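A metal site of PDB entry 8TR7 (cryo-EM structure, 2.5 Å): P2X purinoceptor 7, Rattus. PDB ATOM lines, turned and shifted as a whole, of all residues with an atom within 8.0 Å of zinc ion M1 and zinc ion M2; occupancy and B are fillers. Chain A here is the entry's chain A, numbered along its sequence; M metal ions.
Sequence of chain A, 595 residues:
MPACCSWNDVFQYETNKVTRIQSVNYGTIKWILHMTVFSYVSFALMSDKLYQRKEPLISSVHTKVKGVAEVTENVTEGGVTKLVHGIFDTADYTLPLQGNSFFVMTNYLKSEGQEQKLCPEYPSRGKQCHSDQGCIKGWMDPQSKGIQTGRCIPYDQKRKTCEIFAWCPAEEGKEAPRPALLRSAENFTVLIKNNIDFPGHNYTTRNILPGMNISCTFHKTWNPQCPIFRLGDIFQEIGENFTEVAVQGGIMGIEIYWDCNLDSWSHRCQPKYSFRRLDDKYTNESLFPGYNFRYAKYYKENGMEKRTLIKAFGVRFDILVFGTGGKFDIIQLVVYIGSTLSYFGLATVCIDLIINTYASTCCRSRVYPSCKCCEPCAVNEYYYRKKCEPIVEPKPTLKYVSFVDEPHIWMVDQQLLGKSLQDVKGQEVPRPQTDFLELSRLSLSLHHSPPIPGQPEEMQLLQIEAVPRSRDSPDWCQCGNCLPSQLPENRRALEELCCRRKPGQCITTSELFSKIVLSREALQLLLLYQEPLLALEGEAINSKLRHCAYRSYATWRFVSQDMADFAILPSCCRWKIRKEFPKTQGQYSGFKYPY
The nearest printed residue that does not touch zinc ion M1 is Cys 498 (4.4 Å).
Zinc ion M2 is bound by SG of Cys 482 (2.3 Å). SG of Cys 477 binds zinc ion M2, at 2.3 Å. Zinc ion M2 is bound by the side-chain sulfur (SG) of Cys 498, 2.3 Å away. Zinc ion M2 is bound by the side-chain sulfur (SG) of Cys 479 (2.3 Å). Zinc ion M2 has four donor atoms within binding distance.
Of the 28 residues printed, 4 come within 4 Å of zinc ion M2.
Zinc ion M1 is bound by the side-chain sulfur (SG) of Cys 506, the side-chain sulfur (SG) of Cys 479, the side-chain sulfur (SG) of Cys 572 and the side-chain sulfur (SG) of Cys 499.
SG of Cys 477 sits close to N of Gly 480 (3.6 Å). The side-chain sulfur (SG) of Cys 506 lies close to the side-chain amide oxygen (OD1) of Asn 481 (3.6 Å). O of Cys 499 sits at hydrogen-bond distance from N of Val 404 (3.1 Å). O of Cys 479 lies close to OD1 of Asn 481 (2.9 Å). The side-chain sulfur of Cys 506 sits close to the side-chain hydroxyl of Thr 508, at 3.2 Å. SG of Cys 572 lies close to SG of Cys 573, at 3.7 Å. SG of Cys 482 sits close to N of Cys 572, at 3.3 Å. The backbone NH of Cys 498 is in hydrogen-bond range of the side-chain amide oxygen of Gln 422, 2.5 Å away.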
ATOM      1  N   VAL A 404       8.091 -32.366  25.360  1.00  0.00           N
ATOM      2  CA  VAL A 404       9.451 -32.576  24.891  1.00  0.00           C
ATOM      3  C   VAL A 404      10.420 -31.633  25.606  1.00  0.00           C
ATOM      4  O   VAL A 404      11.564 -31.992  25.893  1.00  0.00           O
ATOM      5  CB  VAL A 404       9.512 -32.409  23.359  1.00  0.00           C
ATOM      6  CG1 VAL A 404       9.287 -30.970  22.978  1.00  0.00           C
ATOM      7  CG2 VAL A 404      10.837 -32.912  22.827  1.00  0.00           C
ATOM      8  N   GLN A 422      -4.080 -29.318  28.293  1.00  0.00           N
ATOM      9  CA  GLN A 422      -2.828 -28.577  28.326  1.00  0.00           C
ATOM     10  C   GLN A 422      -2.749 -27.688  29.559  1.00  0.00           C
ATOM     11  O   GLN A 422      -1.695 -27.612  30.216  1.00  0.00           O
ATOM     12  CB  GLN A 422      -2.694 -27.740  27.058  1.00  0.00           C
ATOM     13  CG  GLN A 422      -1.375 -27.010  26.893  1.00  0.00           C
ATOM     14  CD  GLN A 422      -0.317 -27.818  26.182  1.00  0.00           C
ATOM     15  OE1 GLN A 422      -0.610 -28.631  25.310  1.00  0.00           O
ATOM     16  NE2 GLN A 422       0.938 -27.577  26.544  1.00  0.00           N
ATOM     17  N   SER A 473      -3.762 -21.109  14.490  1.00  0.00           N
ATOM     18  CA  SER A 473      -3.637 -22.294  15.311  1.00  0.00           C
ATOM     19  C   SER A 473      -4.235 -22.043  16.694  1.00  0.00           C
ATOM     20  O   SER A 473      -4.377 -20.905  17.124  1.00  0.00           O
ATOM     21  CB  SER A 473      -2.167 -22.691  15.442  1.00  0.00           C
ATOM     22  OG  SER A 473      -1.545 -22.022  16.531  1.00  0.00           O
ATOM     23  N   PRO A 474      -4.598 -23.118  17.403  1.00  0.00           N
ATOM     24  CA  PRO A 474      -5.234 -22.928  18.715  1.00  0.00           C
ATOM     25  C   PRO A 474      -4.311 -22.195  19.676  1.00  0.00           C
ATOM     26  O   PRO A 474      -3.086 -22.293  19.601  1.00  0.00           O
ATOM     27  CB  PRO A 474      -5.504 -24.360  19.182  1.00  0.00           C
ATOM     28  CG  PRO A 474      -5.439 -25.198  17.962  1.00  0.00           C
ATOM     29  CD  PRO A 474      -4.479 -24.536  17.046  1.00  0.00           C
ATOM     30  N   TRP A 476      -3.874 -22.686  22.896  1.00  0.00           N
ATOM     31  CA  TRP A 476      -3.128 -23.586  23.754  1.00  0.00           C
ATOM     32  C   TRP A 476      -1.938 -24.209  23.044  1.00  0.00           C
ATOM     33  O   TRP A 476      -0.999 -24.659  23.707  1.00  0.00           O
ATOM     34  CB  TRP A 476      -4.046 -24.695  24.293  1.00  0.00           C
ATOM     35  CG  TRP A 476      -4.859 -25.412  23.262  1.00  0.00           C
ATOM     36  CD1 TRP A 476      -6.182 -25.214  22.988  1.00  0.00           C
ATOM     37  CD2 TRP A 476      -4.422 -26.444  22.379  1.00  0.00           C
ATOM     38  NE1 TRP A 476      -6.589 -26.059  21.987  1.00  0.00           N
ATOM     39  CE2 TRP A 476      -5.526 -26.825  21.588  1.00  0.00           C
ATOM     40  CE3 TRP A 476      -3.195 -27.088  22.181  1.00  0.00           C
ATOM     41  CZ2 TRP A 476      -5.435 -27.813  20.620  1.00  0.00           C
ATOM     42  CZ3 TRP A 476      -3.108 -28.063  21.214  1.00  0.00           C
ATOM     43  CH2 TRP A 476      -4.229 -28.423  20.445  1.00  0.00           C
ATOM     44  N   CYS A 477      -1.941 -24.238  21.712  1.00  0.00           N
ATOM     45  CA  CYS A 477      -0.827 -24.779  20.956  1.00  0.00           C
ATOM     46  C   CYS A 477       0.227 -23.718  20.705  1.00  0.00           C
ATOM     47  O   CYS A 477      -0.075 -22.527  20.583  1.00  0.00           O
ATOM     48  CB  CYS A 477      -1.296 -25.348  19.616  1.00  0.00           C
ATOM     49  SG  CYS A 477       0.060 -25.727  18.469  1.00  0.00           S
ATOM     50  N   GLN A 478       1.478 -24.166  20.627  1.00  0.00           N
ATOM     51  CA  GLN A 478       2.586 -23.300  20.259  1.00  0.00           C
ATOM     52  C   GLN A 478       3.591 -23.975  19.338  1.00  0.00           C
ATOM     53  O   GLN A 478       4.633 -23.383  19.043  1.00  0.00           O
ATOM     54  CB  GLN A 478       3.307 -22.784  21.502  1.00  0.00           C
ATOM     55  CG  GLN A 478       3.569 -23.859  22.522  1.00  0.00           C
ATOM     56  CD  GLN A 478       2.502 -23.897  23.591  1.00  0.00           C
ATOM     57  OE1 GLN A 478       1.401 -23.379  23.411  1.00  0.00           O
ATOM     58  NE2 GLN A 478       2.828 -24.504  24.725  1.00  0.00           N
ATOM     59  N   CYS A 479       3.317 -25.198  18.876  1.00  0.00           N
ATOM     60  CA  CYS A 479       4.206 -25.882  17.950  1.00  0.00           C
ATOM     61  C   CYS A 479       3.835 -25.625  16.490  1.00  0.00           C
ATOM     62  O   CYS A 479       4.576 -26.059  15.601  1.00  0.00           O
ATOM     63  CB  CYS A 479       4.196 -27.383  18.233  1.00  0.00           C
ATOM     64  SG  CYS A 479       2.766 -28.296  17.597  1.00  0.00           S
ATOM     65  N   GLY A 480       2.730 -24.930  16.234  1.00  0.00           N
ATOM     66  CA  GLY A 480       2.361 -24.578  14.883  1.00  0.00           C
ATOM     67  C   GLY A 480       1.816 -25.699  14.040  1.00  0.00           C
ATOM     68  O   GLY A 480       1.679 -25.535  12.823  1.00  0.00           O
ATOM     69  N   ASN A 481       1.487 -26.840  14.646  1.00  0.00           N
ATOM     70  CA  ASN A 481       1.015 -28.003  13.901  1.00  0.00           C
ATOM     71  C   ASN A 481      -0.279 -28.604  14.428  1.00  0.00           C
ATOM     72  O   ASN A 481      -0.925 -29.348  13.689  1.00  0.00           O
ATOM     73  CB  ASN A 481       2.097 -29.093  13.892  1.00  0.00           C
ATOM     74  CG  ASN A 481       3.408 -28.618  13.317  1.00  0.00           C
ATOM     75  OD1 ASN A 481       4.394 -28.463  14.048  1.00  0.00           O
ATOM     76  ND2 ASN A 481       3.436 -28.377  12.020  1.00  0.00           N
ATOM     77  N   CYS A 482      -0.676 -28.298  15.660  1.00  0.00           N
ATOM     78  CA  CYS A 482      -1.886 -28.876  16.218  1.00  0.00           C
ATOM     79  C   CYS A 482      -3.122 -28.300  15.537  1.00  0.00           C
ATOM     80  O   CYS A 482      -3.091 -27.216  14.943  1.00  0.00           O
ATOM     81  CB  CYS A 482      -1.953 -28.617  17.714  1.00  0.00           C
ATOM     82  SG  CYS A 482      -0.682 -29.458  18.674  1.00  0.00           S
ATOM     83  N   LEU A 483      -4.218 -29.049  15.605  1.00  0.00           N
ATOM     84  CA  LEU A 483      -5.485 -28.680  14.992  1.00  0.00           C
ATOM     85  C   LEU A 483      -6.601 -28.848  16.003  1.00  0.00           C
ATOM     86  O   LEU A 483      -6.483 -29.607  16.971  1.00  0.00           O
ATOM     87  CB  LEU A 483      -5.769 -29.547  13.765  1.00  0.00           C
ATOM     88  CG  LEU A 483      -4.726 -29.535  12.639  1.00  0.00           C
ATOM     89  CD1 LEU A 483      -5.123 -30.495  11.537  1.00  0.00           C
ATOM     90  CD2 LEU A 483      -4.532 -28.133  12.088  1.00  0.00           C
ATOM     91  N   LEU A 497      -4.338 -31.008  23.419  1.00  0.00           N
ATOM     92  CA  LEU A 497      -3.038 -31.082  24.061  1.00  0.00           C
ATOM     93  C   LEU A 497      -1.948 -30.866  23.011  1.00  0.00           C
ATOM     94  O   LEU A 497      -2.084 -31.312  21.869  1.00  0.00           O
ATOM     95  CB  LEU A 497      -2.843 -32.431  24.757  1.00  0.00           C
ATOM     96  CG  LEU A 497      -1.506 -32.701  25.427  1.00  0.00           C
ATOM     97  CD1 LEU A 497      -1.413 -32.061  26.796  1.00  0.00           C
ATOM     98  CD2 LEU A 497      -1.312 -34.179  25.520  1.00  0.00           C
ATOM     99  N   CYS A 498      -0.886 -30.186  23.411  1.00  0.00           N
ATOM    100  CA  CYS A 498       0.257 -29.925  22.549  1.00  0.00           C
ATOM    101  C   CYS A 498       1.446 -30.774  22.976  1.00  0.00           C
ATOM    102  O   CYS A 498       1.419 -31.490  23.985  1.00  0.00           O
ATOM    103  CB  CYS A 498       0.633 -28.446  22.578  1.00  0.00           C
ATOM    104  SG  CYS A 498       1.642 -27.901  21.186  1.00  0.00           S
ATOM    105  N   CYS A 499       2.511 -30.670  22.191  1.00  0.00           N
ATOM    106  CA  CYS A 499       3.740 -31.396  22.425  1.00  0.00           C
ATOM    107  C   CYS A 499       4.700 -30.684  23.371  1.00  0.00           C
ATOM    108  O   CYS A 499       5.725 -31.264  23.739  1.00  0.00           O
ATOM    109  CB  CYS A 499       4.431 -31.667  21.088  1.00  0.00           C
ATOM    110  SG  CYS A 499       4.909 -30.196  20.168  1.00  0.00           S
ATOM    111  N   ARG A 500       4.399 -29.457  23.796  1.00  0.00           N
ATOM    112  CA  ARG A 500       5.278 -28.727  24.689  1.00  0.00           C
ATOM    113  C   ARG A 500       4.505 -27.640  25.417  1.00  0.00           C
ATOM    114  O   ARG A 500       3.457 -27.191  24.967  1.00  0.00           O
ATOM    115  CB  ARG A 500       6.463 -28.120  23.925  1.00  0.00           C
ATOM    116  CG  ARG A 500       6.063 -27.361  22.677  1.00  0.00           C
ATOM    117  CD  ARG A 500       7.287 -26.985  21.847  1.00  0.00           C
ATOM    118  NE  ARG A 500       8.417 -26.605  22.678  1.00  0.00           N
ATOM    119  CZ  ARG A 500       9.693 -26.757  22.325  1.00  0.00           C
ATOM    120  NH1 ARG A 500      10.021 -27.276  21.159  1.00  0.00           N
ATOM    121  NH2 ARG A 500      10.641 -26.376  23.164  1.00  0.00           N
ATOM    122  N   GLY A 504       8.263 -23.357  20.592  1.00  0.00           N
ATOM    123  CA  GLY A 504       9.458 -23.985  20.076  1.00  0.00           C
ATOM    124  C   GLY A 504       9.114 -24.867  18.892  1.00  0.00           C
ATOM    125  O   GLY A 504       8.019 -24.802  18.332  1.00  0.00           O
ATOM    126  N   GLN A 505      10.084 -25.699  18.524  1.00  0.00           N
ATOM    127  CA  GLN A 505       9.913 -26.616  17.405  1.00  0.00           C
ATOM    128  C   GLN A 505       9.137 -27.846  17.841  1.00  0.00           C
ATOM    129  O   GLN A 505       9.330 -28.366  18.944  1.00  0.00           O
ATOM    130  CB  GLN A 505      11.267 -27.025  16.831  1.00  0.00           C
ATOM    131  CG  GLN A 505      12.260 -27.520  17.866  1.00  0.00           C
ATOM    132  CD  GLN A 505      13.479 -28.164  17.245  1.00  0.00           C
ATOM    133  OE1 GLN A 505      13.436 -28.626  16.107  1.00  0.00           O
ATOM    134  NE2 GLN A 505      14.575 -28.197  17.996  1.00  0.00           N
ATOM    135  N   CYS A 506       8.256 -28.316  16.957  1.00  0.00           N
ATOM    136  CA  CYS A 506       7.454 -29.493  17.247  1.00  0.00           C
ATOM    137  C   CYS A 506       8.336 -30.731  17.333  1.00  0.00           C
ATOM    138  O   CYS A 506       9.354 -30.851  16.650  1.00  0.00           O
ATOM    139  CB  CYS A 506       6.402 -29.695  16.161  1.00  0.00           C
ATOM    140  SG  CYS A 506       5.191 -30.968  16.537  1.00  0.00           S
ATOM    141  N   ILE A 507       7.930 -31.665  18.202  1.00  0.00           N
ATOM    142  CA  ILE A 507       8.648 -32.929  18.317  1.00  0.00           C
ATOM    143  C   ILE A 507       8.614 -33.681  17.003  1.00  0.00           C
ATOM    144  O   ILE A 507       9.588 -34.358  16.642  1.00  0.00           O
ATOM    145  CB  ILE A 507       8.050 -33.774  19.462  1.00  0.00           C
ATOM    146  CG1 ILE A 507       8.929 -34.990  19.735  1.00  0.00           C
ATOM    147  CG2 ILE A 507       6.649 -34.230  19.098  1.00  0.00           C
ATOM    148  CD1 ILE A 507       8.579 -35.709  21.008  1.00  0.00           C
ATOM    149  N   THR A 508       7.512 -33.583  16.266  1.00  0.00           N
ATOM    150  CA  THR A 508       7.348 -34.339  15.040  1.00  0.00           C
ATOM    151  C   THR A 508       8.333 -33.909  13.955  1.00  0.00           C
ATOM    152  O   THR A 508       8.497 -34.633  12.967  1.00  0.00           O
ATOM    153  CB  THR A 508       5.922 -34.200  14.514  1.00  0.00           C
ATOM    154  OG1 THR A 508       5.736 -32.882  13.986  1.00  0.00           O
ATOM    155  CG2 THR A 508       4.908 -34.427  15.607  1.00  0.00           C
ATOM    156  N   THR A 509       8.973 -32.751  14.106  1.00  0.00           N
ATOM    157  CA  THR A 509       9.941 -32.322  13.102  1.00  0.00           C
ATOM    158  C   THR A 509      11.168 -33.221  13.099  1.00  0.00           C
ATOM    159  O   THR A 509      11.880 -33.291  12.087  1.00  0.00           O
ATOM    160  CB  THR A 509      10.355 -30.879  13.372  1.00  0.00           C
ATOM    161  OG1 THR A 509      10.728 -30.716  14.743  1.00  0.00           O
ATOM    162  CG2 THR A 509       9.204 -29.933  13.044  1.00  0.00           C
ATOM    163  N   TYR A 553       4.446 -44.183  19.413  1.00  0.00           N
ATOM    164  CA  TYR A 553       4.686 -42.898  20.084  1.00  0.00           C
ATOM    165  C   TYR A 553       4.554 -43.039  21.589  1.00  0.00           C
ATOM    166  O   TYR A 553       5.377 -42.525  22.358  1.00  0.00           O
ATOM    167  CB  TYR A 553       3.731 -41.832  19.556  1.00  0.00           C
ATOM    168  CG  TYR A 553       3.865 -40.524  20.308  1.00  0.00           C
ATOM    169  CD1 TYR A 553       4.762 -39.554  19.889  1.00  0.00           C
ATOM    170  CD2 TYR A 553       3.112 -40.277  21.437  1.00  0.00           C
ATOM    171  CE1 TYR A 553       4.892 -38.379  20.574  1.00  0.00           C
ATOM    172  CE2 TYR A 553       3.239 -39.104  22.131  1.00  0.00           C
ATOM    173  CZ  TYR A 553       4.132 -38.150  21.697  1.00  0.00           C
ATOM    174  OH  TYR A 553       4.258 -36.977  22.391  1.00  0.00           O
ATOM    175  N   PRO A 570      -0.334 -35.881  21.649  1.00  0.00           N
ATOM    176  CA  PRO A 570      -0.557 -34.506  21.220  1.00  0.00           C
ATOM    177  C   PRO A 570      -1.366 -34.438  19.943  1.00  0.00           C
ATOM    178  O   PRO A 570      -1.349 -35.358  19.119  1.00  0.00           O
ATOM    179  CB  PRO A 570       0.853 -33.951  21.030  1.00  0.00           C
ATOM    180  CG  PRO A 570       1.722 -34.824  21.836  1.00  0.00           C
ATOM    181  CD  PRO A 570       1.101 -36.174  21.816  1.00  0.00           C
ATOM    182  N   SER A 571      -2.093 -33.334  19.776  1.00  0.00           N
ATOM    183  CA  SER A 571      -2.920 -33.169  18.593  1.00  0.00           C
ATOM    184  C   SER A 571      -2.081 -33.171  17.325  1.00  0.00           C
ATOM    185  O   SER A 571      -2.464 -33.757  16.308  1.00  0.00           O
ATOM    186  CB  SER A 571      -3.724 -31.876  18.706  1.00  0.00           C
ATOM    187  OG  SER A 571      -4.512 -31.666  17.546  1.00  0.00           O
ATOM    188  N   CYS A 572      -0.915 -32.519  17.351  1.00  0.00           N
ATOM    189  CA  CYS A 572      -0.045 -32.482  16.189  1.00  0.00           C
ATOM    190  C   CYS A 572       0.319 -33.895  15.738  1.00  0.00           C
ATOM    191  O   CYS A 572       0.123 -34.263  14.575  1.00  0.00           O
ATOM    192  CB  CYS A 572       1.203 -31.660  16.498  1.00  0.00           C
ATOM    193  SG  CYS A 572       2.033 -32.039  18.071  1.00  0.00           S
ATOM    194  N   CYS A 573       0.838 -34.698  16.668  1.00  0.00           N
ATOM    195  CA  CYS A 573       1.262 -36.054  16.336  1.00  0.00           C
ATOM    196  C   CYS A 573       0.079 -36.911  15.898  1.00  0.00           C
ATOM    197  O   CYS A 573       0.178 -37.671  14.924  1.00  0.00           O
ATOM    198  CB  CYS A 573       1.955 -36.663  17.540  1.00  0.00           C
ATOM    199  SG  CYS A 573       3.144 -35.559  18.320  1.00  0.00           S
ATOM    200  N   LYS A 576      -1.060 -35.832  12.402  1.00  0.00           N
ATOM    201  CA  LYS A 576      -0.049 -36.252  11.429  1.00  0.00           C
ATOM    202  C   LYS A 576      -0.158 -37.743  11.145  1.00  0.00           C
ATOM    203  O   LYS A 576      -0.132 -38.166   9.984  1.00  0.00           O
ATOM    204  CB  LYS A 576       1.325 -35.905  11.961  1.00  0.00           C
ATOM    205  CG  LYS A 576       2.463 -36.149  10.994  1.00  0.00           C
ATOM    206  CD  LYS A 576       3.789 -35.771  11.617  1.00  0.00           C
ATOM    207  CE  LYS A 576       3.940 -34.269  11.765  1.00  0.00           C
ATOM    208  NZ  LYS A 576       4.027 -33.542  10.477  1.00  0.00           N
HETATM  209 ZN    ZN M   1       3.665 -30.364  18.182  1.00  0.00          ZN
HETATM  210 ZN    ZN M   2       0.940 -27.823  18.966  1.00  0.00          ZN
